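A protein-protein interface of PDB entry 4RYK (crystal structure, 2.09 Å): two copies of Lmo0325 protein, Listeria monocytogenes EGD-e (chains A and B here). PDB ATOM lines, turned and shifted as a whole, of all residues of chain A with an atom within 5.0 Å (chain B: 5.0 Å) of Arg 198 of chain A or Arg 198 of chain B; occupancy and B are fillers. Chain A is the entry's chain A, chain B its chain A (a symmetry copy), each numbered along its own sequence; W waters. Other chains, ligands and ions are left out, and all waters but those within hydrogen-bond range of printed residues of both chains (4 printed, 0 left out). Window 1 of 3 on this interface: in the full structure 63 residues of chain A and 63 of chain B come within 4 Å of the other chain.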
ATOM      1  N   ASP A  65      22.789   4.084   5.427  1.00  0.00           N
ATOM      2  CA  ASP A  65      21.783   4.568   6.348  1.00  0.00           C
ATOM      3  C   ASP A  65      20.577   5.155   5.577  1.00  0.00           C
ATOM      4  O   ASP A  65      19.457   5.089   6.061  1.00  0.00           O
ATOM      5  CB  ASP A  65      22.378   5.673   7.215  1.00  0.00           C
ATOM      6  CG  ASP A  65      21.455   6.083   8.355  1.00  0.00           C
ATOM      7  OD1 ASP A  65      21.311   5.246   9.292  1.00  0.00           O
ATOM      8  OD2 ASP A  65      20.912   7.228   8.351  1.00  0.00           O
ATOM      9  N   THR A  77      15.321   5.730  11.531  1.00  0.00           N
ATOM     10  CA  THR A  77      16.737   5.463  11.284  1.00  0.00           C
ATOM     11  C   THR A  77      17.276   4.341  12.216  1.00  0.00           C
ATOM     12  O   THR A  77      18.474   4.090  12.223  1.00  0.00           O
ATOM     13  CB  THR A  77      17.617   6.741  11.416  1.00  0.00           C
ATOM     14  OG1 THR A  77      17.655   7.196  12.791  1.00  0.00           O
ATOM     15  CG2 THR A  77      17.099   7.852  10.496  1.00  0.00           C
ATOM     16  N   GLU A  78      16.409   3.686  12.994  1.00  0.00           N
ATOM     17  CA  GLU A  78      16.747   2.421  13.684  1.00  0.00           C
ATOM     18  C   GLU A  78      15.647   1.327  13.510  1.00  0.00           C
ATOM     19  O   GLU A  78      14.429   1.587  13.545  1.00  0.00           O
ATOM     20  CB  GLU A  78      17.038   2.639  15.194  1.00  0.00           C
ATOM     21  CG  GLU A  78      18.296   3.452  15.547  1.00  0.00           C
ATOM     22  CD  GLU A  78      18.056   4.969  15.547  1.00  0.00           C
ATOM     23  OE1 GLU A  78      17.185   5.385  16.368  1.00  0.00           O
ATOM     24  OE2 GLU A  78      18.716   5.733  14.744  1.00  0.00           O
ATOM     25  N   TYR A 196      30.420  11.754  16.221  1.00  0.00           N
ATOM     26  CA  TYR A 196      29.329  11.022  15.613  1.00  0.00           C
ATOM     27  C   TYR A 196      28.083  11.938  15.735  1.00  0.00           C
ATOM     28  O   TYR A 196      27.698  12.373  16.818  1.00  0.00           O
ATOM     29  CB  TYR A 196      29.147   9.682  16.313  1.00  0.00           C
ATOM     30  CG  TYR A 196      28.057   8.758  15.795  1.00  0.00           C
ATOM     31  CD1 TYR A 196      27.824   8.583  14.432  1.00  0.00           C
ATOM     32  CD2 TYR A 196      27.324   7.987  16.678  1.00  0.00           C
ATOM     33  CE1 TYR A 196      26.827   7.733  13.986  1.00  0.00           C
ATOM     34  CE2 TYR A 196      26.332   7.148  16.245  1.00  0.00           C
ATOM     35  CZ  TYR A 196      26.091   7.013  14.904  1.00  0.00           C
ATOM     36  OH  TYR A 196      25.091   6.151  14.523  1.00  0.00           O
ATOM     37  N   ASP A 197      27.496  12.300  14.612  1.00  0.00           N
ATOM     38  CA  ASP A 197      26.350  13.212  14.649  1.00  0.00           C
ATOM     39  C   ASP A 197      25.312  12.764  15.661  1.00  0.00           C
ATOM     40  O   ASP A 197      24.932  13.543  16.526  1.00  0.00           O
ATOM     41  CB  ASP A 197      25.749  13.485  13.245  1.00  0.00           C
ATOM     42  CG  ASP A 197      25.240  12.249  12.536  1.00  0.00           C
ATOM     43  OD1 ASP A 197      25.327  11.095  12.987  1.00  0.00           O
ATOM     44  OD2 ASP A 197      24.736  12.456  11.434  1.00  0.00           O
ATOM     45  N   ARG A 198      24.941  11.496  15.643  1.00  0.00           N
ATOM     46  CA  ARG A 198      23.905  11.020  16.573  1.00  0.00           C
ATOM     47  C   ARG A 198      24.406  10.917  18.010  1.00  0.00           C
ATOM     48  O   ARG A 198      23.667  11.190  18.947  1.00  0.00           O
ATOM     49  CB  ARG A 198      23.332   9.677  16.096  1.00  0.00           C
ATOM     50  CG  ARG A 198      22.400   9.916  14.906  1.00  0.00           C
ATOM     51  CD  ARG A 198      22.042   8.668  14.151  1.00  0.00           C
ATOM     52  NE  ARG A 198      21.393   9.055  12.916  1.00  0.00           N
ATOM     53  CZ  ARG A 198      21.221   8.277  11.861  1.00  0.00           C
ATOM     54  NH1 ARG A 198      21.581   7.014  11.901  1.00  0.00           N
ATOM     55  NH2 ARG A 198      20.673   8.765  10.754  1.00  0.00           N
ATOM     56  N   GLY A 199      25.655  10.535  18.187  1.00  0.00           N
ATOM     57  CA  GLY A 199      26.166  10.321  19.511  1.00  0.00           C
ATOM     58  C   GLY A 199      26.386  11.638  20.164  1.00  0.00           C
ATOM     59  O   GLY A 199      26.161  11.804  21.339  1.00  0.00           O
ATOM     60  N   ARG A 200      26.828  12.605  19.390  1.00  0.00           N
ATOM     61  CA  ARG A 200      27.068  13.922  19.943  1.00  0.00           C
ATOM     62  C   ARG A 200      25.843  14.506  20.643  1.00  0.00           C
ATOM     63  O   ARG A 200      25.937  15.041  21.745  1.00  0.00           O
ATOM     64  CB  ARG A 200      27.607  14.831  18.858  1.00  0.00           C
ATOM     65  CG  ARG A 200      27.628  16.293  19.209  1.00  0.00           C
ATOM     66  CD  ARG A 200      28.453  17.056  18.205  1.00  0.00           C
ATOM     67  NE  ARG A 200      27.891  17.015  16.874  1.00  0.00           N
ATOM     68  CZ  ARG A 200      28.474  16.485  15.830  1.00  0.00           C
ATOM     69  NH1 ARG A 200      29.597  15.864  15.964  1.00  0.00           N
ATOM     70  NH2 ARG A 200      27.884  16.522  14.644  1.00  0.00           N
ATOM     71  N   LEU A 201      24.683  14.382  20.056  1.00  0.00           N
ATOM     72  CA  LEU A 201      23.491  14.967  20.655  1.00  0.00           C
ATOM     73  C   LEU A 201      23.040  14.192  21.906  1.00  0.00           C
ATOM     74  O   LEU A 201      22.560  14.772  22.863  1.00  0.00           O
ATOM     75  CB  LEU A 201      22.324  14.983  19.642  1.00  0.00           C
ATOM     76  CG  LEU A 201      22.569  15.796  18.337  1.00  0.00           C
ATOM     77  CD1 LEU A 201      21.362  15.716  17.368  1.00  0.00           C
ATOM     78  CD2 LEU A 201      22.870  17.252  18.658  1.00  0.00           C
ATOM     79  N   LEU A 202      23.194  12.885  21.888  1.00  0.00           N
ATOM     80  CA  LEU A 202      22.944  12.078  23.104  1.00  0.00           C
ATOM     81  C   LEU A 202      23.882  12.468  24.228  1.00  0.00           C
ATOM     82  O   LEU A 202      23.454  12.655  25.344  1.00  0.00           O
ATOM     83  CB  LEU A 202      23.159  10.645  22.766  1.00  0.00           C
ATOM     84  CG  LEU A 202      22.880   9.675  23.905  1.00  0.00           C
ATOM     85  CD1 LEU A 202      21.396   9.640  24.236  1.00  0.00           C
ATOM     86  CD2 LEU A 202      23.383   8.277  23.502  1.00  0.00           C
ATOM     87  N   ASP B  65      23.997   1.774  12.047  1.00  0.00           N
ATOM     88  CA  ASP B  65      24.812   2.927  11.733  1.00  0.00           C
ATOM     89  C   ASP B  65      25.928   3.109  12.789  1.00  0.00           C
ATOM     90  O   ASP B  65      26.999   3.599  12.461  1.00  0.00           O
ATOM     91  CB  ASP B  65      23.942   4.180  11.738  1.00  0.00           C
ATOM     92  CG  ASP B  65      24.675   5.404  11.203  1.00  0.00           C
ATOM     93  OD1 ASP B  65      24.915   5.418   9.962  1.00  0.00           O
ATOM     94  OD2 ASP B  65      24.973   6.357  11.984  1.00  0.00           O
ATOM     95  N   THR B  77      30.496   8.431   9.018  1.00  0.00           N
ATOM     96  CA  THR B  77      29.187   7.787   8.928  1.00  0.00           C
ATOM     97  C   THR B  77      28.818   7.451   7.456  1.00  0.00           C
ATOM     98  O   THR B  77      27.699   7.027   7.198  1.00  0.00           O
ATOM     99  CB  THR B  77      28.058   8.638   9.584  1.00  0.00           C
ATOM    100  OG1 THR B  77      27.826   9.850   8.826  1.00  0.00           O
ATOM    101  CG2 THR B  77      28.408   8.971  11.038  1.00  0.00           C
ATOM    102  N   GLU B  78      29.739   7.643   6.506  1.00  0.00           N
ATOM    103  CA  GLU B  78      29.613   7.085   5.141  1.00  0.00           C
ATOM    104  C   GLU B  78      30.922   6.389   4.653  1.00  0.00           C
ATOM    105  O   GLU B  78      32.056   6.850   4.884  1.00  0.00           O
ATOM    106  CB  GLU B  78      29.172   8.159   4.109  1.00  0.00           C
ATOM    107  CG  GLU B  78      27.753   8.731   4.269  1.00  0.00           C
ATOM    108  CD  GLU B  78      27.679   9.899   5.264  1.00  0.00           C
ATOM    109  OE1 GLU B  78      28.383  10.911   4.972  1.00  0.00           O
ATOM    110  OE2 GLU B  78      26.940   9.812   6.318  1.00  0.00           O
ATOM    111  N   TYR B 196      14.181  12.834   8.189  1.00  0.00           N
ATOM    112  CA  TYR B 196      15.440  12.124   8.262  1.00  0.00           C
ATOM    113  C   TYR B 196      16.462  13.131   8.853  1.00  0.00           C
ATOM    114  O   TYR B 196      16.669  14.227   8.336  1.00  0.00           O
ATOM    115  CB  TYR B 196      15.837  11.622   6.880  1.00  0.00           C
ATOM    116  CG  TYR B 196      17.127  10.828   6.762  1.00  0.00           C
ATOM    117  CD1 TYR B 196      17.493   9.869   7.705  1.00  0.00           C
ATOM    118  CD2 TYR B 196      17.934  10.976   5.648  1.00  0.00           C
ATOM    119  CE1 TYR B 196      18.672   9.156   7.573  1.00  0.00           C
ATOM    120  CE2 TYR B 196      19.104  10.279   5.512  1.00  0.00           C
ATOM    121  CZ  TYR B 196      19.468   9.365   6.466  1.00  0.00           C
ATOM    122  OH  TYR B 196      20.647   8.686   6.276  1.00  0.00           O
ATOM    123  N   ASP B 197      17.046  12.795   9.985  1.00  0.00           N
ATOM    124  CA  ASP B 197      17.978  13.723  10.630  1.00  0.00           C
ATOM    125  C   ASP B 197      19.005  14.254   9.649  1.00  0.00           C
ATOM    126  O   ASP B 197      19.153  15.463   9.519  1.00  0.00           O
ATOM    127  CB  ASP B 197      18.614  13.143  11.920  1.00  0.00           C
ATOM    128  CG  ASP B 197      19.415  11.878  11.703  1.00  0.00           C
ATOM    129  OD1 ASP B 197      19.530  11.298  10.610  1.00  0.00           O
ATOM    130  OD2 ASP B 197      19.948  11.423  12.713  1.00  0.00           O
ATOM    131  N   ARG B 198      19.626  13.382   8.874  1.00  0.00           N
ATOM    132  CA  ARG B 198      20.665  13.840   7.937  1.00  0.00           C
ATOM    133  C   ARG B 198      20.089  14.586   6.738  1.00  0.00           C
ATOM    134  O   ARG B 198      20.684  15.540   6.256  1.00  0.00           O
ATOM    135  CB  ARG B 198      21.532  12.657   7.479  1.00  0.00           C
ATOM    136  CG  ARG B 198      22.483  12.257   8.610  1.00  0.00           C
ATOM    137  CD  ARG B 198      23.142  10.923   8.408  1.00  0.00           C
ATOM    138  NE  ARG B 198      23.790  10.545   9.647  1.00  0.00           N
ATOM    139  CZ  ARG B 198      24.195   9.327   9.962  1.00  0.00           C
ATOM    140  NH1 ARG B 198      24.096   8.347   9.092  1.00  0.00           N
ATOM    141  NH2 ARG B 198      24.714   9.086  11.161  1.00  0.00           N
ATOM    142  N   GLY B 199      18.933  14.165   6.264  1.00  0.00           N
ATOM    143  CA  GLY B 199      18.378  14.756   5.079  1.00  0.00           C
ATOM    144  C   GLY B 199      17.847  16.104   5.414  1.00  0.00           C
ATOM    145  O   GLY B 199      17.946  17.027   4.642  1.00  0.00           O
ATOM    146  N   ARG B 200      17.277  16.230   6.592  1.00  0.00           N
ATOM    147  CA  ARG B 200      16.735  17.509   7.000  1.00  0.00           C
ATOM    148  C   ARG B 200      17.760  18.639   6.935  1.00  0.00           C
ATOM    149  O   ARG B 200      17.477  19.723   6.433  1.00  0.00           O
ATOM    150  CB  ARG B 200      16.106  17.373   8.371  1.00  0.00           C
ATOM    151  CG  ARG B 200      15.763  18.673   9.043  1.00  0.00           C
ATOM    152  CD  ARG B 200      14.878  18.423  10.237  1.00  0.00           C
ATOM    153  NE  ARG B 200      15.535  17.650  11.267  1.00  0.00           N
ATOM    154  CZ  ARG B 200      15.151  16.468  11.677  1.00  0.00           C
ATOM    155  NH1 ARG B 200      14.170  15.868  11.091  1.00  0.00           N
ATOM    156  NH2 ARG B 200      15.809  15.852  12.648  1.00  0.00           N
ATOM    157  N   LEU B 201      18.962  18.404   7.389  1.00  0.00           N
ATOM    158  CA  LEU B 201      19.962  19.463   7.398  1.00  0.00           C
ATOM    159  C   LEU B 201      20.465  19.788   5.981  1.00  0.00           C
ATOM    160  O   LEU B 201      20.744  20.929   5.661  1.00  0.00           O
ATOM    161  CB  LEU B 201      21.174  19.060   8.268  1.00  0.00           C
ATOM    162  CG  LEU B 201      20.868  18.770   9.767  1.00  0.00           C
ATOM    163  CD1 LEU B 201      22.135  18.333  10.544  1.00  0.00           C
ATOM    164  CD2 LEU B 201      20.255  19.991  10.437  1.00  0.00           C
ATOM    165  N   LEU B 202      20.582  18.780   5.142  1.00  0.00           N
ATOM    166  CA  LEU B 202      20.898  19.018   3.715  1.00  0.00           C
ATOM    167  C   LEU B 202      19.818  19.839   3.040  1.00  0.00           C
ATOM    168  O   LEU B 202      20.115  20.783   2.342  1.00  0.00           O
ATOM    169  CB  LEU B 202      21.004  17.699   3.035  1.00  0.00           C
ATOM    170  CG  LEU B 202      21.388  17.773   1.564  1.00  0.00           C
ATOM    171  CD1 LEU B 202      22.819  18.261   1.400  1.00  0.00           C
ATOM    172  CD2 LEU B 202      21.210  16.380   0.933  1.00  0.00           C
HETATM  173  O   HOH W   1      18.075   9.740  13.753  1.00  0.00           O
HETATM  174  O   HOH W   2      25.386   5.601   5.736  1.00  0.00           O
HETATM  175  O   HOH W   3      26.828  12.262   9.699  1.00  0.00           O
HETATM  176  O   HOH W   4      21.130   2.565  12.593  1.00  0.00           O
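Printed residues of chain B within 4 Å of Asp 65 of chain A: Asp 65, Tyr 196 and Arg 198. Of the printed residues of chain B, Asp 197 of chain A touches Arg 198 (2.8 Å). Of the printed residues of chain A, Asp 65 of chain B touches Asp 65, Tyr 196 and Arg 198. Of the printed residues of chain A, Thr 77 of chain B touches Tyr 196 (3.5 Å). Printed residues of chain A within 4 Å of Tyr 196 of chain B: Asp 65 (2.5 Å), Thr 77 (3.5 Å) and Arg 198 (3.8 Å). Of chain A, only Asp 65, Tyr 196, Asp 197 and Arg 198 come within 4 Å of Arg 198 of chain B. Leu 202 of chain B touches none of the printed residues of chain A. The nearest printed residue of chain B that does not touch Arg 198 of chain A is Thr 77 of chain B (6.3 Å). The nearest printed residue of chain A that does not touch Arg 198 of chain B is Thr 77 of chain A (6.3 Å). The nearest printed residue of chain B that does not touch Tyr 196 of chain A is Asp 197 of chain B (7.6 Å).
Among the printed residues, merely in contact across the chains: Tyr 196 of chain A with Thr 77 of chain B (3.5 Å), Thr 77 of chain A with Tyr 196 of chain B (3.5 Å), Arg 198 of chain A with Arg 198 of chain B (3.7 Å), Asp 65 of chain A with Asp 65 of chain B (3.7 Å), Arg 198 of chain A with Tyr 196 of chain B (3.8 Å) and Tyr 196 of chain A with Arg 198 of chain B (3.8 Å).
Of the 10 printed residues of chain A, 5 touch a printed residue of chain B. Hydrophobic or aromatic side chains of chain A that line the printed part of chain B: Tyr 196. Of the 10 printed residues of chain B, 5 touch a printed residue of chain A. Hydrophobic or aromatic side chains of chain B that line the printed part of chain A: Tyr 196. Among the printed residues, Asp or Glu carboxylates within 4 Å of a Lys or Arg side-chain nitrogen of the other chain: Asp 65 of chain A with Arg 198 of chain B, Asp 197 of chain A with Arg 198 of chain B, Arg 198 of chain A with Asp 65 of chain B and Arg 198 of chain A with Asp 197 of chain B.
OD2 of Asp 65 of chain A lies within salt-bridge range of NH2 of Arg 198 of chain A (2.9 Å). OG1 of Thr 77 of chain A is in hydrogen-bond range of OE2 of Glu 78 of chain A, at 2.7 Å. OD2 of Asp 65 of chain B is in salt-bridge range of NH2 of Arg 198 of chain B (2.9 Å). The side-chain hydroxyl of Thr 77 of chain B lies within hydrogen-bond range of the side-chain carboxylate of Glu 78 of chain B.
Thr 77 of chain A touches Tyr 196 of chain B, and with the chains exchanged Tyr 196 of chain A touches Thr 77 of chain B. Tyr 196 of chain A touches Arg 198 of chain B, and with the chains exchanged Arg 198 of chain A touches Tyr 196 of chain B. Asp 197 of chain A touches Arg 198 of chain B, and with the chains exchanged Arg 198 of chain A touches Asp 197 of chain B. Arg 198 of chain B touches its own counterpart, Arg 198 of chain A. 10 positions are printed for both chains.
The side-chain hydroxyl (OH) of Tyr 196 of chain B is in hydrogen-bond range of the side-chain carboxylate (OD2) of Asp 65 of chain A. OD2 of Asp 65 of chain A lies within salt-bridge range of NH1 of Arg 198 of chain B (3.5 Å). The side-chain hydroxyl (OH) of Tyr 196 of chain A sits at hydrogen-bond distance from the side-chain carboxylate (OD2) of Asp 65 of chain B (2.6 Å). The side-chain carboxylate of Asp 197 of chain A lies within salt-bridge range of the guanidinium group of Arg 198 of chain B (2.8 Å). OD2 of Asp 65 of chain B lies within salt-bridge range of NH1 of Arg 198 of chain A (3.5 Å). OD2 of Asp 197 of chain B is in salt-bridge range of NE of Arg 198 of chain A (2.8 Å).
Water W1 lies within hydrogen-bond range of the side-chain carboxylate of Asp 197 of chain B (2.7 Å), the side-chain hydroxyl of Thr 77 of chain A (2.8 Å) and the guanidinium group of Arg 198 of chain A (3.5 Å). Water W3 lies within hydrogen-bond range of OD2 of Asp 197 of chain A (2.7 Å), OG1 of Thr 77 of chain B (2.8 Å) and NE of Arg 198 of chain B (3.5 Å). Water W2 bridges the backbone NH of Asp 65 of chain A (3.0 Å) and the backbone carbonyl oxygen of Thr 77 of chain B (3.1 Å). Water W4 lies within hydrogen-bond range of N of Asp 65 of chain B and O of Thr 77 of chain A.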
